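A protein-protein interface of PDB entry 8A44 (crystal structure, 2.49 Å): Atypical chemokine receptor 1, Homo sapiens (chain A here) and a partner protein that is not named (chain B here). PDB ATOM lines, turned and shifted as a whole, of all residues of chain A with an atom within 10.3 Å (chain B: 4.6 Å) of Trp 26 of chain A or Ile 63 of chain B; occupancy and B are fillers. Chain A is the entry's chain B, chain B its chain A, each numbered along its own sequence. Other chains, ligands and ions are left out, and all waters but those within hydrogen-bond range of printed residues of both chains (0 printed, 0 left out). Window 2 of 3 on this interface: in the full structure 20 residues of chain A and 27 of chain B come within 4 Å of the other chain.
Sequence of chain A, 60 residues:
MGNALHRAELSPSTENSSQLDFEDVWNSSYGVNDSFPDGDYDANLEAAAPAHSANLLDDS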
ATOM      1  N   LEU A  20       9.717  -1.080  -8.976  1.00  0.00           N
ATOM      2  CA  LEU A  20      11.006  -1.758  -8.945  1.00  0.00           C
ATOM      3  C   LEU A  20      12.016  -1.038  -9.831  1.00  0.00           C
ATOM      4  O   LEU A  20      11.661  -0.424 -10.842  1.00  0.00           O
ATOM      5  CB  LEU A  20      10.865  -3.205  -9.422  1.00  0.00           C
ATOM      6  CG  LEU A  20       9.876  -4.046  -8.614  1.00  0.00           C
ATOM      7  CD1 LEU A  20       9.109  -5.000  -9.517  1.00  0.00           C
ATOM      8  CD2 LEU A  20      10.590  -4.800  -7.516  1.00  0.00           C
ATOM      9  N   ASP A  21      13.289  -1.122  -9.445  1.00  0.00           N
ATOM     10  CA  ASP A  21      14.386  -0.674 -10.309  1.00  0.00           C
ATOM     11  C   ASP A  21      14.561  -1.740 -11.387  1.00  0.00           C
ATOM     12  O   ASP A  21      15.226  -2.758 -11.168  1.00  0.00           O
ATOM     13  CB  ASP A  21      15.663  -0.458  -9.496  1.00  0.00           C
ATOM     14  CG  ASP A  21      16.886  -0.101 -10.357  1.00  0.00           C
ATOM     15  OD1 ASP A  21      16.771   0.157 -11.585  1.00  0.00           O
ATOM     16  OD2 ASP A  21      17.993  -0.066  -9.776  1.00  0.00           O
ATOM     17  N   PHE A  22      13.948  -1.519 -12.554  1.00  0.00           N
ATOM     18  CA  PHE A  22      13.888  -2.586 -13.542  1.00  0.00           C
ATOM     19  C   PHE A  22      15.242  -2.863 -14.163  1.00  0.00           C
ATOM     20  O   PHE A  22      15.464  -3.972 -14.652  1.00  0.00           O
ATOM     21  CB  PHE A  22      12.827  -2.264 -14.598  1.00  0.00           C
ATOM     22  CG  PHE A  22      11.414  -2.495 -14.098  1.00  0.00           C
ATOM     23  CD1 PHE A  22      10.638  -1.428 -13.643  1.00  0.00           C
ATOM     24  CD2 PHE A  22      10.872  -3.779 -14.066  1.00  0.00           C
ATOM     25  CE1 PHE A  22       9.361  -1.637 -13.174  1.00  0.00           C
ATOM     26  CE2 PHE A  22       9.595  -3.990 -13.603  1.00  0.00           C
ATOM     27  CZ  PHE A  22       8.840  -2.920 -13.149  1.00  0.00           C
ATOM     28  N   GLU A  23      16.176  -1.916 -14.113  1.00  0.00           N
ATOM     29  CA  GLU A  23      17.502  -2.260 -14.598  1.00  0.00           C
ATOM     30  C   GLU A  23      18.169  -3.244 -13.652  1.00  0.00           C
ATOM     31  O   GLU A  23      18.845  -4.177 -14.099  1.00  0.00           O
ATOM     32  CB  GLU A  23      18.357  -1.016 -14.793  1.00  0.00           C
ATOM     33  CG  GLU A  23      19.591  -1.344 -15.615  1.00  0.00           C
ATOM     34  CD  GLU A  23      20.619  -0.236 -15.656  1.00  0.00           C
ATOM     35  OE1 GLU A  23      20.367   0.776 -16.343  1.00  0.00           O
ATOM     36  OE2 GLU A  23      21.677  -0.378 -14.997  1.00  0.00           O
ATOM     37  N   ASP A  24      17.958  -3.079 -12.343  1.00  0.00           N
ATOM     38  CA  ASP A  24      18.500  -4.044 -11.394  1.00  0.00           C
ATOM     39  C   ASP A  24      17.860  -5.420 -11.565  1.00  0.00           C
ATOM     40  O   ASP A  24      18.539  -6.447 -11.447  1.00  0.00           O
ATOM     41  CB  ASP A  24      18.315  -3.545  -9.964  1.00  0.00           C
ATOM     42  CG  ASP A  24      19.202  -4.282  -8.994  1.00  0.00           C
ATOM     43  OD1 ASP A  24      20.397  -4.455  -9.323  1.00  0.00           O
ATOM     44  OD2 ASP A  24      18.714  -4.704  -7.923  1.00  0.00           O
ATOM     45  N   VAL A  25      16.551  -5.464 -11.819  1.00  0.00           N
ATOM     46  CA  VAL A  25      15.879  -6.735 -12.061  1.00  0.00           C
ATOM     47  C   VAL A  25      16.568  -7.482 -13.194  1.00  0.00           C
ATOM     48  O   VAL A  25      16.871  -8.676 -13.085  1.00  0.00           O
ATOM     49  CB  VAL A  25      14.389  -6.508 -12.376  1.00  0.00           C
ATOM     50  CG1 VAL A  25      13.713  -7.849 -12.689  1.00  0.00           C
ATOM     51  CG2 VAL A  25      13.686  -5.799 -11.235  1.00  0.00           C
ATOM     52  N   TRP A  26      16.824  -6.774 -14.299  1.00  0.00           N
ATOM     53  CA  TRP A  26      17.424  -7.381 -15.483  1.00  0.00           C
ATOM     54  C   TRP A  26      18.808  -7.947 -15.172  1.00  0.00           C
ATOM     55  O   TRP A  26      19.082  -9.123 -15.445  1.00  0.00           O
ATOM     56  CB  TRP A  26      17.496  -6.349 -16.610  1.00  0.00           C
ATOM     57  CG  TRP A  26      18.295  -6.840 -17.740  1.00  0.00           C
ATOM     58  CD1 TRP A  26      19.612  -6.604 -17.973  1.00  0.00           C
ATOM     59  CD2 TRP A  26      17.848  -7.703 -18.789  1.00  0.00           C
ATOM     60  NE1 TRP A  26      20.012  -7.250 -19.110  1.00  0.00           N
ATOM     61  CE2 TRP A  26      18.947  -7.938 -19.630  1.00  0.00           C
ATOM     62  CE3 TRP A  26      16.618  -8.292 -19.105  1.00  0.00           C
ATOM     63  CZ2 TRP A  26      18.861  -8.747 -20.768  1.00  0.00           C
ATOM     64  CZ3 TRP A  26      16.532  -9.096 -20.245  1.00  0.00           C
ATOM     65  CH2 TRP A  26      17.646  -9.308 -21.061  1.00  0.00           C
ATOM     66  N   ASN A  27      19.689  -7.115 -14.593  1.00  0.00           N
ATOM     67  CA  ASN A  27      21.029  -7.554 -14.203  1.00  0.00           C
ATOM     68  C   ASN A  27      20.999  -8.697 -13.191  1.00  0.00           C
ATOM     69  O   ASN A  27      21.944  -9.496 -13.142  1.00  0.00           O
ATOM     70  CB  ASN A  27      21.832  -6.393 -13.607  1.00  0.00           C
ATOM     71  CG  ASN A  27      22.163  -5.306 -14.628  1.00  0.00           C
ATOM     72  OD1 ASN A  27      22.471  -5.582 -15.795  1.00  0.00           O
ATOM     73  ND2 ASN A  27      22.159  -4.058 -14.165  1.00  0.00           N
ATOM     74  N   SER A  28      19.952  -8.774 -12.360  1.00  0.00           N
ATOM     75  CA  SER A  28      19.853  -9.816 -11.345  1.00  0.00           C
ATOM     76  C   SER A  28      19.407 -11.157 -11.903  1.00  0.00           C
ATOM     77  O   SER A  28      19.625 -12.189 -11.259  1.00  0.00           O
ATOM     78  CB  SER A  28      18.868  -9.401 -10.255  1.00  0.00           C
ATOM     79  OG  SER A  28      19.186  -8.109  -9.777  1.00  0.00           O
ATOM     80  N   SER A  29      18.772 -11.168 -13.065  1.00  0.00           N
ATOM     81  CA  SER A  29      18.141 -12.390 -13.522  1.00  0.00           C
ATOM     82  C   SER A  29      19.135 -13.394 -14.087  1.00  0.00           C
ATOM     83  O   SER A  29      18.764 -14.554 -14.276  1.00  0.00           O
ATOM     84  CB  SER A  29      17.070 -12.058 -14.561  1.00  0.00           C
ATOM     85  OG  SER A  29      17.654 -11.422 -15.682  1.00  0.00           O
ATOM     86  N   TYR A  30      20.379 -13.000 -14.357  1.00  0.00           N
ATOM     87  CA  TYR A  30      21.318 -13.988 -14.868  1.00  0.00           C
ATOM     88  C   TYR A  30      22.747 -13.599 -14.554  1.00  0.00           C
ATOM     89  O   TYR A  30      23.082 -12.413 -14.451  1.00  0.00           O
ATOM     90  CB  TYR A  30      21.147 -14.211 -16.371  1.00  0.00           C
ATOM     91  CG  TYR A  30      21.595 -13.114 -17.320  1.00  0.00           C
ATOM     92  CD1 TYR A  30      21.034 -11.836 -17.274  1.00  0.00           C
ATOM     93  CD2 TYR A  30      22.520 -13.388 -18.326  1.00  0.00           C
ATOM     94  CE1 TYR A  30      21.417 -10.846 -18.183  1.00  0.00           C
ATOM     95  CE2 TYR A  30      22.910 -12.418 -19.239  1.00  0.00           C
ATOM     96  CZ  TYR A  30      22.357 -11.145 -19.170  1.00  0.00           C
ATOM     97  OH  TYR A  30      22.765 -10.187 -20.099  1.00  0.00           O
ATOM     98  N   GLY A  31      23.577 -14.627 -14.395  1.00  0.00           N
ATOM     99  CA  GLY A  31      24.995 -14.489 -14.145  1.00  0.00           C
ATOM    100  C   GLY A  31      25.377 -13.942 -12.791  1.00  0.00           C
ATOM    101  O   GLY A  31      26.575 -13.779 -12.529  1.00  0.00           O
ATOM    102  N   VAL A  32      24.411 -13.651 -11.925  1.00  0.00           N
ATOM    103  CA  VAL A  32      24.705 -13.007 -10.648  1.00  0.00           C
ATOM    104  C   VAL A  32      25.592 -13.932  -9.824  1.00  0.00           C
ATOM    105  O   VAL A  32      26.770 -13.624  -9.598  1.00  0.00           O
ATOM    106  CB  VAL A  32      23.405 -12.605  -9.921  1.00  0.00           C
ATOM    107  CG1 VAL A  32      23.574 -12.583  -8.414  1.00  0.00           C
ATOM    108  CG2 VAL A  32      22.971 -11.238 -10.420  1.00  0.00           C
ATOM    109  N   LEU B  56      15.024 -11.303 -27.678  1.00  0.00           N
ATOM    110  CA  LEU B  56      15.682 -10.589 -26.592  1.00  0.00           C
ATOM    111  C   LEU B  56      14.792  -9.475 -26.063  1.00  0.00           C
ATOM    112  O   LEU B  56      14.763  -9.211 -24.860  1.00  0.00           O
ATOM    113  CB  LEU B  56      17.025 -10.031 -27.070  1.00  0.00           C
ATOM    114  CG  LEU B  56      17.850  -9.323 -25.998  1.00  0.00           C
ATOM    115  CD1 LEU B  56      18.338 -10.316 -24.944  1.00  0.00           C
ATOM    116  CD2 LEU B  56      18.996  -8.576 -26.623  1.00  0.00           C
ATOM    117  N   LYS B  59      12.250 -11.273 -23.954  1.00  0.00           N
ATOM    118  CA  LYS B  59      12.789 -11.676 -22.656  1.00  0.00           C
ATOM    119  C   LYS B  59      12.756 -10.518 -21.671  1.00  0.00           C
ATOM    120  O   LYS B  59      12.294 -10.663 -20.535  1.00  0.00           O
ATOM    121  CB  LYS B  59      14.217 -12.208 -22.781  1.00  0.00           C
ATOM    122  CG  LYS B  59      14.724 -12.691 -21.422  1.00  0.00           C
ATOM    123  CD  LYS B  59      16.149 -13.177 -21.444  1.00  0.00           C
ATOM    124  CE  LYS B  59      16.209 -14.664 -21.761  1.00  0.00           C
ATOM    125  NZ  LYS B  59      17.513 -14.918 -22.446  1.00  0.00           N
ATOM    126  N   ARG B  60      13.244  -9.354 -22.097  1.00  0.00           N
ATOM    127  CA  ARG B  60      13.244  -8.194 -21.217  1.00  0.00           C
ATOM    128  C   ARG B  60      11.831  -7.883 -20.725  1.00  0.00           C
ATOM    129  O   ARG B  60      11.600  -7.728 -19.522  1.00  0.00           O
ATOM    130  CB  ARG B  60      13.844  -7.001 -21.950  1.00  0.00           C
ATOM    131  CG  ARG B  60      14.052  -5.763 -21.085  1.00  0.00           C
ATOM    132  CD  ARG B  60      15.146  -4.890 -21.693  1.00  0.00           C
ATOM    133  NE  ARG B  60      16.233  -4.551 -20.777  1.00  0.00           N
ATOM    134  CZ  ARG B  60      17.527  -4.640 -21.077  1.00  0.00           C
ATOM    135  NH1 ARG B  60      17.941  -5.138 -22.237  1.00  0.00           N
ATOM    136  NH2 ARG B  60      18.430  -4.185 -20.205  1.00  0.00           N
ATOM    137  N   LYS B  61      10.863  -7.828 -21.651  1.00  0.00           N
ATOM    138  CA  LYS B  61       9.489  -7.496 -21.277  1.00  0.00           C
ATOM    139  C   LYS B  61       8.934  -8.524 -20.309  1.00  0.00           C
ATOM    140  O   LYS B  61       8.290  -8.169 -19.311  1.00  0.00           O
ATOM    141  CB  LYS B  61       8.597  -7.401 -22.524  1.00  0.00           C
ATOM    142  CG  LYS B  61       8.870  -6.217 -23.473  1.00  0.00           C
ATOM    143  CD  LYS B  61       8.690  -4.853 -22.785  1.00  0.00           C
ATOM    144  CE  LYS B  61       9.619  -3.761 -23.367  1.00  0.00           C
ATOM    145  NZ  LYS B  61      10.243  -2.835 -22.336  1.00  0.00           N
ATOM    146  N   LEU B  62       9.182  -9.812 -20.585  1.00  0.00           N
ATOM    147  CA  LEU B  62       8.651 -10.873 -19.737  1.00  0.00           C
ATOM    148  C   LEU B  62       9.305 -10.852 -18.359  1.00  0.00           C
ATOM    149  O   LEU B  62       8.634 -11.098 -17.345  1.00  0.00           O
ATOM    150  CB  LEU B  62       8.835 -12.228 -20.429  1.00  0.00           C
ATOM    151  CG  LEU B  62       8.395 -13.475 -19.659  1.00  0.00           C
ATOM    152  CD1 LEU B  62       6.924 -13.396 -19.280  1.00  0.00           C
ATOM    153  CD2 LEU B  62       8.672 -14.742 -20.464  1.00  0.00           C
ATOM    154  N   ILE B  63      10.601 -10.534 -18.297  1.00  0.00           N
ATOM    155  CA  ILE B  63      11.280 -10.414 -17.008  1.00  0.00           C
ATOM    156  C   ILE B  63      10.651  -9.299 -16.162  1.00  0.00           C
ATOM    157  O   ILE B  63      10.449  -9.460 -14.948  1.00  0.00           O
ATOM    158  CB  ILE B  63      12.789 -10.209 -17.237  1.00  0.00           C
ATOM    159  CG1 ILE B  63      13.435 -11.544 -17.583  1.00  0.00           C
ATOM    160  CG2 ILE B  63      13.476  -9.681 -16.009  1.00  0.00           C
ATOM    161  CD1 ILE B  63      14.902 -11.440 -17.904  1.00  0.00           C
ATOM    162  N   TYR B  64      10.299  -8.170 -16.783  1.00  0.00           N
ATOM    163  CA  TYR B  64       9.664  -7.090 -16.030  1.00  0.00           C
ATOM    164  C   TYR B  64       8.310  -7.522 -15.472  1.00  0.00           C
ATOM    165  O   TYR B  64       7.991  -7.241 -14.308  1.00  0.00           O
ATOM    166  CB  TYR B  64       9.499  -5.842 -16.903  1.00  0.00           C
ATOM    167  CG  TYR B  64      10.796  -5.151 -17.291  1.00  0.00           C
ATOM    168  CD1 TYR B  64      12.009  -5.530 -16.723  1.00  0.00           C
ATOM    169  CD2 TYR B  64      10.812  -4.118 -18.245  1.00  0.00           C
ATOM    170  CE1 TYR B  64      13.203  -4.901 -17.087  1.00  0.00           C
ATOM    171  CE2 TYR B  64      11.997  -3.488 -18.607  1.00  0.00           C
ATOM    172  CZ  TYR B  64      13.189  -3.885 -18.025  1.00  0.00           C
ATOM    173  OH  TYR B  64      14.383  -3.286 -18.373  1.00  0.00           O
ATOM    174  N   ASP B  65       7.498  -8.206 -16.282  1.00  0.00           N
ATOM    175  CA  ASP B  65       6.181  -8.631 -15.804  1.00  0.00           C
ATOM    176  C   ASP B  65       6.305  -9.689 -14.720  1.00  0.00           C
ATOM    177  O   ASP B  65       5.530  -9.689 -13.750  1.00  0.00           O
ATOM    178  CB  ASP B  65       5.332  -9.160 -16.956  1.00  0.00           C
ATOM    179  CG  ASP B  65       4.658  -8.038 -17.754  1.00  0.00           C
ATOM    180  OD1 ASP B  65       4.122  -8.324 -18.858  1.00  0.00           O
ATOM    181  OD2 ASP B  65       4.674  -6.870 -17.299  1.00  0.00           O
ATOM    182  N   ALA B  66       7.276 -10.598 -14.863  1.00  0.00           N
ATOM    183  CA  ALA B  66       7.481 -11.613 -13.836  1.00  0.00           C
ATOM    184  C   ALA B  66       7.985 -10.987 -12.542  1.00  0.00           C
ATOM    185  O   ALA B  66       7.577 -11.397 -11.453  1.00  0.00           O
ATOM    186  CB  ALA B  66       8.452 -12.680 -14.339  1.00  0.00           C
ATOM    187  N   ALA B  67       8.865  -9.989 -12.634  1.00  0.00           N
ATOM    188  CA  ALA B  67       9.312  -9.298 -11.428  1.00  0.00           C
ATOM    189  C   ALA B  67       8.143  -8.635 -10.704  1.00  0.00           C
ATOM    190  O   ALA B  67       8.010  -8.750  -9.476  1.00  0.00           O
ATOM    191  CB  ALA B  67      10.373  -8.263 -11.775  1.00  0.00           C
ATOM    192  N   GLN B 142      15.656 -18.232 -15.734  1.00  0.00           N
ATOM    193  CA  GLN B 142      15.908 -16.802 -15.622  1.00  0.00           C
ATOM    194  C   GLN B 142      14.619 -16.051 -15.313  1.00  0.00           C
ATOM    195  O   GLN B 142      14.627 -15.091 -14.531  1.00  0.00           O
ATOM    196  CB  GLN B 142      16.560 -16.289 -16.901  1.00  0.00           C
ATOM    197  CG  GLN B 142      16.899 -14.812 -16.882  1.00  0.00           C
ATOM    198  CD  GLN B 142      17.541 -14.394 -18.172  1.00  0.00           C
ATOM    199  OE1 GLN B 142      17.535 -15.160 -19.142  1.00  0.00           O
ATOM    200  NE2 GLN B 142      18.098 -13.176 -18.209  1.00  0.00           N
ATOM    201  N   ILE B 143      13.495 -16.495 -15.890  1.00  0.00           N
ATOM    202  CA  ILE B 143      12.226 -15.858 -15.571  1.00  0.00           C
ATOM    203  C   ILE B 143      11.882 -16.081 -14.111  1.00  0.00           C
ATOM    204  O   ILE B 143      11.391 -15.169 -13.424  1.00  0.00           O
ATOM    205  CB  ILE B 143      11.111 -16.363 -16.494  1.00  0.00           C
ATOM    206  CG1 ILE B 143      11.462 -16.082 -17.953  1.00  0.00           C
ATOM    207  CG2 ILE B 143       9.780 -15.727 -16.115  1.00  0.00           C
ATOM    208  CD1 ILE B 143      11.834 -14.671 -18.234  1.00  0.00           C
ATOM    209  N   ALA B 146      13.751 -13.692 -11.908  1.00  0.00           N
ATOM    210  CA  ALA B 146      13.117 -12.377 -11.870  1.00  0.00           C
ATOM    211  C   ALA B 146      11.912 -12.361 -10.934  1.00  0.00           C
ATOM    212  O   ALA B 146      11.634 -11.334 -10.299  1.00  0.00           O
ATOM    213  CB  ALA B 146      12.701 -11.943 -13.272  1.00  0.00           C
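Leu 20 of chain A touches Ala 67 of chain B (CD1 to O, 3.9 Å). Phe 22 of chain A touches Tyr 64 of chain B (CD2 to CD1, 3.4 Å). Ile 63 of chain B touches Val 25 of chain A. CG1 of Val 25 of chain A touches CB of Ala 67 of chain B, 3.5 Å away. Trp 26 of chain A touches Arg 60 of chain B. Trp 26 of chain A touches Ile 63 of chain B. OG of Ser 29 of chain A touches CD1 of Ile 63 of chain B, at 3.5 Å. Tyr 30 of chain A touches Gln 142 of chain B (CD1 to NE2, 3.4 Å).
Hydrophobic or aromatic side chains of chain A within 4 Å of the printed part of chain B: Leu 20, Phe 22, Val 25, Trp 26 and Tyr 30. Hydrophobic or aromatic side chains of chain B that line the printed part of chain A: Ile 63, Tyr 64 and Ala 67. Among the printed residues, 9 pairs touch across the chains. Among the printed residues, no Asp or Glu carboxylate lies within 4 Å of a Lys or Arg side-chain nitrogen of the other chain.
The side-chain amide nitrogen (NE2) of Gln 142 of chain B sits at hydrogen-bond distance from the side-chain hydroxyl (OG) of Ser 29 of chain A (3.1 Å).
The side-chain amino group of Lys 59 of chain B lies close to the side-chain amide oxygen of Gln 142 of chain B. The guanidinium group (NE) of Arg 60 of chain B is in hydrogen-bond range of the side-chain hydroxyl (OH) of Tyr 64 of chain B, 3.3 Å away. The backbone carbonyl oxygen (O) of Trp 26 of chain A sits at hydrogen-bond distance from the side-chain hydroxyl (OG) of Ser 29 of chain A (2.7 Å).
Trp 26 of chain A touches just these residues of chain B: Arg 60 and Ile 63. Ile 63 of chain B touches just these residues of chain A: Val 25 (3.8 Å), Trp 26 (3.7 Å) and Ser 29 (3.5 Å). No residue of chain A comes within 4 Å of Lys 59 of chain B. Of chain A, only Trp 26 (3.5 Å) comes within 4 Å of Arg 60 of chain B. No residue of chain A comes within 4 Å of Leu 62 of chain B. No residue of chain A comes within 4 Å of Ala 66 of chain B. Ala 67 of chain B touches two residues of chain A. No residue of chain A comes within 4 Å of Ile 143 of chain B. No residue of chain A comes within 4 Å of Ala 146 of chain B. Printed residues of chain B within 4 Å of Phe 22 of chain A: Tyr 64 (3.4 Å). Of the printed residues of chain A, Tyr 64 of chain B touches Phe 22 (3.4 Å). Of the printed residues of chain B, Val 25 of chain A touches Ile 63 (3.8 Å) and Ala 67 (3.5 Å). Of the printed residues of chain B, Tyr 30 of chain A touches Gln 142 (3.4 Å). Of the printed residues of chain B, Ser 29 of chain A touches Ile 63 and Gln 142. Asp 21 of chain A touches none of the printed residues of chain B. Asn 27 of chain A touches none of the printed residues of chain B. The nearest residue of chain B that does not touch Trp 26 of chain A is Leu 56 of chain B (4.1 Å). The nearest residue of chain A that does not touch Ile 63 of chain B is Phe 22 of chain A (5.7 Å).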
